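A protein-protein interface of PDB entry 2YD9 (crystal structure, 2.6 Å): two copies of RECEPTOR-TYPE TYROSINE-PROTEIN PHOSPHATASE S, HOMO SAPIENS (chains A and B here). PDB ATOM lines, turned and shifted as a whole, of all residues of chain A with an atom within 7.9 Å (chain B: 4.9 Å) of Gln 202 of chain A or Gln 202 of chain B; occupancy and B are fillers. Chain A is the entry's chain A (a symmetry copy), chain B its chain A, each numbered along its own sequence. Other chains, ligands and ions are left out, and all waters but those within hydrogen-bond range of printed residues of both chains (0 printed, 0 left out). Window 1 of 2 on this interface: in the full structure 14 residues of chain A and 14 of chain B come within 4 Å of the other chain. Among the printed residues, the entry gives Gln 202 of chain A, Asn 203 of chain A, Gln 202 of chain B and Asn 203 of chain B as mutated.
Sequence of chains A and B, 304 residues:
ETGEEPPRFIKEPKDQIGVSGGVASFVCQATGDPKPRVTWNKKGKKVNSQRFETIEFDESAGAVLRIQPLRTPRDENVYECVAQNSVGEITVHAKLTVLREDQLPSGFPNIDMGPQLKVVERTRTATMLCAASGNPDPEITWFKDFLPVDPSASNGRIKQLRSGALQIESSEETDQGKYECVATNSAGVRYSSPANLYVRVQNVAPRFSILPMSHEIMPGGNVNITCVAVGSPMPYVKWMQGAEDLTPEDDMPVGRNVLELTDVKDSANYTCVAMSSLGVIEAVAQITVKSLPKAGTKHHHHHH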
ATOM      1  N   GLU A 121     -14.228 -18.124  18.712  1.00  0.00           N
ATOM      2  CA  GLU A 121     -13.179 -18.361  19.703  1.00  0.00           C
ATOM      3  C   GLU A 121     -11.903 -18.739  18.958  1.00  0.00           C
ATOM      4  O   GLU A 121     -11.970 -19.249  17.842  1.00  0.00           O
ATOM      5  CB  GLU A 121     -13.594 -19.413  20.746  1.00  0.00           C
ATOM      6  CG  GLU A 121     -14.391 -18.827  21.938  1.00  0.00           C
ATOM      7  CD  GLU A 121     -15.876 -18.591  21.631  1.00  0.00           C
ATOM      8  OE1 GLU A 121     -16.512 -19.552  21.163  1.00  0.00           O
ATOM      9  OE2 GLU A 121     -16.422 -17.483  21.881  1.00  0.00           O
ATOM     10  N   ARG A 122     -10.750 -18.449  19.561  1.00  0.00           N
ATOM     11  CA  ARG A 122      -9.455 -18.662  18.908  1.00  0.00           C
ATOM     12  C   ARG A 122      -9.294 -20.122  18.512  1.00  0.00           C
ATOM     13  O   ARG A 122      -9.742 -21.013  19.227  1.00  0.00           O
ATOM     14  CB  ARG A 122      -8.290 -18.253  19.819  1.00  0.00           C
ATOM     15  CG  ARG A 122      -7.109 -17.662  19.058  1.00  0.00           C
ATOM     16  CD  ARG A 122      -5.767 -18.146  19.560  1.00  0.00           C
ATOM     17  NE  ARG A 122      -5.562 -17.899  20.988  1.00  0.00           N
ATOM     18  CZ  ARG A 122      -5.452 -18.838  21.932  1.00  0.00           C
ATOM     19  NH1 ARG A 122      -5.525 -20.141  21.637  1.00  0.00           N
ATOM     20  NH2 ARG A 122      -5.262 -18.469  23.197  1.00  0.00           N
ATOM     21  N   ARG A 124     -10.872 -21.691  16.330  1.00  0.00           N
ATOM     22  CA  ARG A 124     -12.113 -22.214  15.768  1.00  0.00           C
ATOM     23  C   ARG A 124     -12.345 -21.667  14.367  1.00  0.00           C
ATOM     24  O   ARG A 124     -11.688 -20.714  13.946  1.00  0.00           O
ATOM     25  CB  ARG A 124     -13.286 -21.854  16.671  1.00  0.00           C
ATOM     26  CG  ARG A 124     -13.198 -22.458  18.077  1.00  0.00           C
ATOM     27  CD  ARG A 124     -13.543 -23.934  18.072  1.00  0.00           C
ATOM     28  NE  ARG A 124     -14.891 -24.146  17.545  1.00  0.00           N
ATOM     29  CZ  ARG A 124     -16.001 -24.291  18.275  1.00  0.00           C
ATOM     30  NH1 ARG A 124     -15.968 -24.278  19.605  1.00  0.00           N
ATOM     31  NH2 ARG A 124     -17.165 -24.470  17.661  1.00  0.00           N
ATOM     32  N   VAL A 199     -12.396 -12.163  17.361  1.00  0.00           N
ATOM     33  CA  VAL A 199     -11.714 -13.405  17.742  1.00  0.00           C
ATOM     34  C   VAL A 199     -11.457 -13.432  19.243  1.00  0.00           C
ATOM     35  O   VAL A 199     -10.637 -12.671  19.763  1.00  0.00           O
ATOM     36  CB  VAL A 199     -10.376 -13.608  16.992  1.00  0.00           C
ATOM     37  CG1 VAL A 199      -9.676 -14.852  17.497  1.00  0.00           C
ATOM     38  CG2 VAL A 199     -10.613 -13.722  15.492  1.00  0.00           C
ATOM     39  N   ARG A 200     -12.155 -14.335  19.925  1.00  0.00           N
ATOM     40  CA  ARG A 200     -12.147 -14.404  21.379  1.00  0.00           C
ATOM     41  C   ARG A 200     -11.013 -15.282  21.913  1.00  0.00           C
ATOM     42  O   ARG A 200     -10.945 -16.485  21.634  1.00  0.00           O
ATOM     43  CB  ARG A 200     -13.497 -14.944  21.872  1.00  0.00           C
ATOM     44  CG  ARG A 200     -13.611 -15.136  23.376  1.00  0.00           C
ATOM     45  CD  ARG A 200     -14.067 -13.882  24.048  1.00  0.00           C
ATOM     46  NE  ARG A 200     -14.054 -13.994  25.506  1.00  0.00           N
ATOM     47  CZ  ARG A 200     -13.170 -13.411  26.315  1.00  0.00           C
ATOM     48  NH1 ARG A 200     -12.184 -12.657  25.833  1.00  0.00           N
ATOM     49  NH2 ARG A 200     -13.274 -13.578  27.631  1.00  0.00           N
ATOM     50  N   VAL A 201     -10.136 -14.665  22.696  1.00  0.00           N
ATOM     51  CA  VAL A 201      -9.168 -15.390  23.494  1.00  0.00           C
ATOM     52  C   VAL A 201      -9.683 -15.432  24.930  1.00  0.00           C
ATOM     53  O   VAL A 201     -10.073 -14.406  25.486  1.00  0.00           O
ATOM     54  CB  VAL A 201      -7.792 -14.718  23.452  1.00  0.00           C
ATOM     55  CG1 VAL A 201      -6.799 -15.483  24.303  1.00  0.00           C
ATOM     56  CG2 VAL A 201      -7.303 -14.618  22.018  1.00  0.00           C
ATOM     57  N   GLN A 202      -9.702 -16.631  25.507  1.00  0.00           N
ATOM     58  CA  GLN A 202     -10.095 -16.846  26.900  1.00  0.00           C
ATOM     59  C   GLN A 202      -8.848 -17.167  27.714  1.00  0.00           C
ATOM     60  O   GLN A 202      -8.354 -18.291  27.669  1.00  0.00           O
ATOM     61  CB  GLN A 202     -11.075 -18.017  26.992  1.00  0.00           C
ATOM     62  CG  GLN A 202     -12.419 -17.766  26.371  1.00  0.00           C
ATOM     63  CD  GLN A 202     -13.310 -18.989  26.441  1.00  0.00           C
ATOM     64  OE1 GLN A 202     -13.203 -19.900  25.620  1.00  0.00           O
ATOM     65  NE2 GLN A 202     -14.197 -19.012  27.418  1.00  0.00           N
ATOM     66  N   ASN A 203      -8.336 -16.186  28.451  1.00  0.00           N
ATOM     67  CA  ASN A 203      -7.055 -16.341  29.137  1.00  0.00           C
ATOM     68  C   ASN A 203      -6.991 -15.632  30.482  1.00  0.00           C
ATOM     69  O   ASN A 203      -6.066 -14.856  30.736  1.00  0.00           O
ATOM     70  CB  ASN A 203      -5.916 -15.848  28.241  1.00  0.00           C
ATOM     71  CG  ASN A 203      -4.561 -16.371  28.683  1.00  0.00           C
ATOM     72  OD1 ASN A 203      -4.379 -17.577  28.853  1.00  0.00           O
ATOM     73  ND2 ASN A 203      -3.604 -15.470  28.857  1.00  0.00           N
ATOM     74  N   VAL A 204      -7.978 -15.909  31.333  1.00  0.00           N
ATOM     75  CA  VAL A 204      -8.004 -15.382  32.690  1.00  0.00           C
ATOM     76  C   VAL A 204      -8.093 -16.531  33.691  1.00  0.00           C
ATOM     77  O   VAL A 204      -9.065 -17.302  33.692  1.00  0.00           O
ATOM     78  CB  VAL A 204      -9.170 -14.391  32.886  1.00  0.00           C
ATOM     79  CG1 VAL A 204      -9.276 -13.962  34.351  1.00  0.00           C
ATOM     80  CG2 VAL A 204      -8.982 -13.178  31.974  1.00  0.00           C
ATOM     81  N   ALA A 205      -7.062 -16.646  34.531  1.00  0.00           N
ATOM     82  CA  ALA A 205      -6.966 -17.725  35.523  1.00  0.00           C
ATOM     83  C   ALA A 205      -8.061 -17.561  36.561  1.00  0.00           C
ATOM     84  O   ALA A 205      -8.435 -16.442  36.882  1.00  0.00           O
ATOM     85  CB  ALA A 205      -5.610 -17.716  36.187  1.00  0.00           C
ATOM     86  N   GLY A 231     -13.515 -16.270  35.973  1.00  0.00           N
ATOM     87  CA  GLY A 231     -12.351 -16.464  35.096  1.00  0.00           C
ATOM     88  C   GLY A 231     -12.785 -16.755  33.672  1.00  0.00           C
ATOM     89  O   GLY A 231     -13.964 -16.966  33.412  1.00  0.00           O
ATOM     90  N   SER A 232     -11.831 -16.787  32.745  1.00  0.00           N
ATOM     91  CA  SER A 232     -12.134 -17.006  31.329  1.00  0.00           C
ATOM     92  C   SER A 232     -11.133 -17.982  30.733  1.00  0.00           C
ATOM     93  O   SER A 232     -10.002 -17.604  30.435  1.00  0.00           O
ATOM     94  CB  SER A 232     -12.099 -15.686  30.565  1.00  0.00           C
ATOM     95  OG  SER A 232     -12.563 -15.861  29.238  1.00  0.00           O
ATOM     96  N   PRO A 233     -11.537 -19.245  30.539  1.00  0.00           N
ATOM     97  CA  PRO A 233     -12.871 -19.805  30.713  1.00  0.00           C
ATOM     98  C   PRO A 233     -13.366 -19.802  32.156  1.00  0.00           C
ATOM     99  O   PRO A 233     -12.594 -19.599  33.087  1.00  0.00           O
ATOM    100  CB  PRO A 233     -12.726 -21.227  30.181  1.00  0.00           C
ATOM    101  CG  PRO A 233     -11.317 -21.548  30.330  1.00  0.00           C
ATOM    102  CD  PRO A 233     -10.567 -20.276  30.146  1.00  0.00           C
ATOM    103  N   MET A 234     -14.664 -20.007  32.319  1.00  0.00           N
ATOM    104  CA  MET A 234     -15.317 -19.936  33.619  1.00  0.00           C
ATOM    105  C   MET A 234     -15.080 -21.271  34.317  1.00  0.00           C
ATOM    106  O   MET A 234     -15.302 -22.322  33.721  1.00  0.00           O
ATOM    107  CB  MET A 234     -16.810 -19.687  33.423  1.00  0.00           C
ATOM    108  CG  MET A 234     -17.504 -19.038  34.595  1.00  0.00           C
ATOM    109  SD  MET A 234     -17.130 -17.283  34.742  1.00  0.00           S
ATOM    110  CE  MET A 234     -18.196 -16.827  36.111  1.00  0.00           C
ATOM    111  N   TYR A 236     -15.221 -24.639  36.781  1.00  0.00           N
ATOM    112  CA  TYR A 236     -16.145 -25.499  37.524  1.00  0.00           C
ATOM    113  C   TYR A 236     -15.989 -25.153  39.004  1.00  0.00           C
ATOM    114  O   TYR A 236     -14.952 -24.621  39.407  1.00  0.00           O
ATOM    115  CB  TYR A 236     -15.812 -26.978  37.343  1.00  0.00           C
ATOM    116  CG  TYR A 236     -16.173 -27.592  36.009  1.00  0.00           C
ATOM    117  CD1 TYR A 236     -17.504 -27.745  35.622  1.00  0.00           C
ATOM    118  CD2 TYR A 236     -15.186 -28.080  35.156  1.00  0.00           C
ATOM    119  CE1 TYR A 236     -17.836 -28.333  34.407  1.00  0.00           C
ATOM    120  CE2 TYR A 236     -15.510 -28.676  33.942  1.00  0.00           C
ATOM    121  CZ  TYR A 236     -16.835 -28.798  33.573  1.00  0.00           C
ATOM    122  OH  TYR A 236     -17.152 -29.391  32.368  1.00  0.00           O
ATOM    123  N   VAL A 254     -20.942 -24.682  37.095  1.00  0.00           N
ATOM    124  CA  VAL A 254     -19.926 -23.751  36.623  1.00  0.00           C
ATOM    125  C   VAL A 254     -20.155 -22.404  37.291  1.00  0.00           C
ATOM    126  O   VAL A 254     -21.260 -21.881  37.262  1.00  0.00           O
ATOM    127  CB  VAL A 254     -19.991 -23.574  35.091  1.00  0.00           C
ATOM    128  CG1 VAL A 254     -19.252 -22.314  34.659  1.00  0.00           C
ATOM    129  CG2 VAL A 254     -19.416 -24.795  34.393  1.00  0.00           C
ATOM    130  N   SER A 277      -9.044 -24.666  32.981  1.00  0.00           N
ATOM    131  CA  SER A 277      -7.839 -25.094  32.282  1.00  0.00           C
ATOM    132  C   SER A 277      -6.635 -24.198  32.591  1.00  0.00           C
ATOM    133  O   SER A 277      -5.506 -24.550  32.251  1.00  0.00           O
ATOM    134  CB  SER A 277      -8.085 -25.158  30.772  1.00  0.00           C
ATOM    135  OG  SER A 277      -8.380 -23.880  30.241  1.00  0.00           O
ATOM    136  N   LEU A 278      -6.876 -23.053  33.231  1.00  0.00           N
ATOM    137  CA  LEU A 278      -5.805 -22.123  33.585  1.00  0.00           C
ATOM    138  C   LEU A 278      -5.414 -22.175  35.065  1.00  0.00           C
ATOM    139  O   LEU A 278      -4.546 -21.411  35.500  1.00  0.00           O
ATOM    140  CB  LEU A 278      -6.206 -20.697  33.200  1.00  0.00           C
ATOM    141  CG  LEU A 278      -6.524 -20.496  31.715  1.00  0.00           C
ATOM    142  CD1 LEU A 278      -6.961 -19.064  31.464  1.00  0.00           C
ATOM    143  CD2 LEU A 278      -5.327 -20.860  30.845  1.00  0.00           C
ATOM    144  N   GLU B 121     -10.334 -27.854  27.877  1.00  0.00           N
ATOM    145  CA  GLU B 121     -11.478 -27.520  27.030  1.00  0.00           C
ATOM    146  C   GLU B 121     -11.467 -28.459  25.829  1.00  0.00           C
ATOM    147  O   GLU B 121     -10.411 -28.962  25.450  1.00  0.00           O
ATOM    148  CB  GLU B 121     -11.485 -26.035  26.626  1.00  0.00           C
ATOM    149  CG  GLU B 121     -12.165 -25.111  27.665  1.00  0.00           C
ATOM    150  CD  GLU B 121     -11.262 -24.749  28.853  1.00  0.00           C
ATOM    151  OE1 GLU B 121     -10.140 -24.287  28.585  1.00  0.00           O
ATOM    152  OE2 GLU B 121     -11.667 -24.885  30.040  1.00  0.00           O
ATOM    153  N   ARG B 200     -14.087 -29.924  29.203  1.00  0.00           N
ATOM    154  CA  ARG B 200     -15.073 -28.854  29.228  1.00  0.00           C
ATOM    155  C   ARG B 200     -15.641 -28.555  27.838  1.00  0.00           C
ATOM    156  O   ARG B 200     -14.915 -28.165  26.918  1.00  0.00           O
ATOM    157  CB  ARG B 200     -14.435 -27.585  29.811  1.00  0.00           C
ATOM    158  CG  ARG B 200     -15.332 -26.357  29.836  1.00  0.00           C
ATOM    159  CD  ARG B 200     -16.149 -26.310  31.087  1.00  0.00           C
ATOM    160  NE  ARG B 200     -17.120 -25.216  31.077  1.00  0.00           N
ATOM    161  CZ  ARG B 200     -18.435 -25.357  30.922  1.00  0.00           C
ATOM    162  NH1 ARG B 200     -18.986 -26.557  30.746  1.00  0.00           N
ATOM    163  NH2 ARG B 200     -19.218 -24.282  30.947  1.00  0.00           N
ATOM    164  N   VAL B 201     -16.951 -28.728  27.710  1.00  0.00           N
ATOM    165  CA  VAL B 201     -17.687 -28.241  26.561  1.00  0.00           C
ATOM    166  C   VAL B 201     -18.392 -26.951  26.969  1.00  0.00           C
ATOM    167  O   VAL B 201     -19.054 -26.899  28.005  1.00  0.00           O
ATOM    168  CB  VAL B 201     -18.716 -29.269  26.079  1.00  0.00           C
ATOM    169  CG1 VAL B 201     -19.482 -28.735  24.886  1.00  0.00           C
ATOM    170  CG2 VAL B 201     -18.026 -30.575  25.730  1.00  0.00           C
ATOM    171  N   GLN B 202     -18.217 -25.911  26.157  1.00  0.00           N
ATOM    172  CA  GLN B 202     -18.876 -24.619  26.355  1.00  0.00           C
ATOM    173  C   GLN B 202     -19.964 -24.462  25.300  1.00  0.00           C
ATOM    174  O   GLN B 202     -19.667 -24.146  24.150  1.00  0.00           O
ATOM    175  CB  GLN B 202     -17.859 -23.485  26.207  1.00  0.00           C
ATOM    176  CG  GLN B 202     -16.821 -23.423  27.290  1.00  0.00           C
ATOM    177  CD  GLN B 202     -15.812 -22.321  27.042  1.00  0.00           C
ATOM    178  OE1 GLN B 202     -14.867 -22.487  26.272  1.00  0.00           O
ATOM    179  NE2 GLN B 202     -16.006 -21.192  27.698  1.00  0.00           N
ATOM    180  N   ASN B 203     -21.217 -24.683  25.684  1.00  0.00           N
ATOM    181  CA  ASN B 203     -22.312 -24.718  24.717  1.00  0.00           C
ATOM    182  C   ASN B 203     -23.620 -24.154  25.252  1.00  0.00           C
ATOM    183  O   ASN B 203     -24.663 -24.810  25.174  1.00  0.00           O
ATOM    184  CB  ASN B 203     -22.533 -26.151  24.225  1.00  0.00           C
ATOM    185  CG  ASN B 203     -23.324 -26.205  22.930  1.00  0.00           C
ATOM    186  OD1 ASN B 203     -22.972 -25.547  21.951  1.00  0.00           O
ATOM    187  ND2 ASN B 203     -24.387 -26.998  22.915  1.00  0.00           N
ATOM    188  N   VAL B 204     -23.552 -22.937  25.789  1.00  0.00           N
ATOM    189  CA  VAL B 204     -24.733 -22.227  26.258  1.00  0.00           C
ATOM    190  C   VAL B 204     -24.841 -20.876  25.554  1.00  0.00           C
ATOM    191  O   VAL B 204     -23.955 -20.019  25.683  1.00  0.00           O
ATOM    192  CB  VAL B 204     -24.710 -22.048  27.791  1.00  0.00           C
ATOM    193  CG1 VAL B 204     -25.879 -21.173  28.251  1.00  0.00           C
ATOM    194  CG2 VAL B 204     -24.749 -23.415  28.476  1.00  0.00           C
ATOM    195  N   SER B 232     -22.048 -19.654  27.928  1.00  0.00           N
ATOM    196  CA  SER B 232     -20.793 -20.409  27.905  1.00  0.00           C
ATOM    197  C   SER B 232     -20.455 -20.804  26.478  1.00  0.00           C
ATOM    198  O   SER B 232     -21.034 -21.746  25.942  1.00  0.00           O
ATOM    199  CB  SER B 232     -20.902 -21.653  28.782  1.00  0.00           C
ATOM    200  OG  SER B 232     -19.644 -22.291  28.908  1.00  0.00           O
ATOM    201  N   PRO B 233     -19.505 -20.099  25.847  1.00  0.00           N
ATOM    202  CA  PRO B 233     -18.644 -19.056  26.387  1.00  0.00           C
ATOM    203  C   PRO B 233     -19.386 -17.792  26.813  1.00  0.00           C
ATOM    204  O   PRO B 233     -20.547 -17.598  26.471  1.00  0.00           O
ATOM    205  CB  PRO B 233     -17.679 -18.770  25.241  1.00  0.00           C
ATOM    206  CG  PRO B 233     -18.390 -19.164  24.037  1.00  0.00           C
ATOM    207  CD  PRO B 233     -19.266 -20.306  24.411  1.00  0.00           C
ATOM    208  N   LEU B 278     -22.094 -18.412  20.022  1.00  0.00           N
ATOM    209  CA  LEU B 278     -23.357 -19.146  19.959  1.00  0.00           C
ATOM    210  C   LEU B 278     -24.576 -18.247  19.729  1.00  0.00           C
ATOM    211  O   LEU B 278     -25.708 -18.741  19.693  1.00  0.00           O
ATOM    212  CB  LEU B 278     -23.546 -19.968  21.236  1.00  0.00           C
ATOM    213  CG  LEU B 278     -22.434 -20.982  21.519  1.00  0.00           C
ATOM    214  CD1 LEU B 278     -22.700 -21.695  22.834  1.00  0.00           C
ATOM    215  CD2 LEU B 278     -22.300 -21.981  20.377  1.00  0.00           C
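OE1 of Glu 121 of chain B sits at hydrogen-bond distance from OG of Ser 277 of chain A (2.5 Å). The side-chain amide nitrogen (NE2) of Gln 202 of chain B sits close to the side-chain amide nitrogen (NE2) of Gln 202 of chain A (2.8 Å).
NH2 of Arg 200 of chain B lies within hydrogen-bond range of OG of Ser 232 of chain B (2.9 Å).
Glu 121 of chain A touches Pro 233 of chain B (OE2 to CG, 3.4 Å). CG of Pro 233 of chain A touches OE2 of Glu 121 of chain B, at 3.4 Å. CD of Arg 200 of chain B touches OH of Tyr 236 of chain A, at 3.5 Å. Val 254 of chain A touches Arg 200 of chain B (CG2 to NH2, 3.5 Å).
Of chain A, only Gln 202 (2.8 Å) comes within 4 Å of Gln 202 of chain B. Printed residues of chain B within 4 Å of Pro 233 of chain A: Glu 121. Printed residues of chain B within 4 Å of Tyr 236 of chain A: Arg 200. Ala 205 of chain A touches none of the printed residues of chain B. Val 204 of chain A touches none of the printed residues of chain B. The nearest printed residue of chain A that does not touch Pro 233 of chain B is Gln 202 of chain A (4.1 Å).
Of the 18 printed residues of chain A, 6 touch a printed residue of chain B. Hydrophobic or aromatic side chains of chain A that line the printed part of chain B: Pro 233, Tyr 236 and Val 254. Along chain A the printed residues that touch a printed residue of chain B span positions 121 to 277. Of the 9 printed residues of chain B, 4 touch a printed residue of chain A. Hydrophobic or aromatic side chains of chain B that line the printed part of chain A: Pro 233.
Glu 121 of chain A touches Pro 233 of chain B, and with the chains exchanged Pro 233 of chain A touches Glu 121 of chain B. Gln 202 of chain A touches its own counterpart, Gln 202 of chain B. Of the 6 pairs that touch across the chains among the printed residues, 3 have their exchanged pair printed and touching as well.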
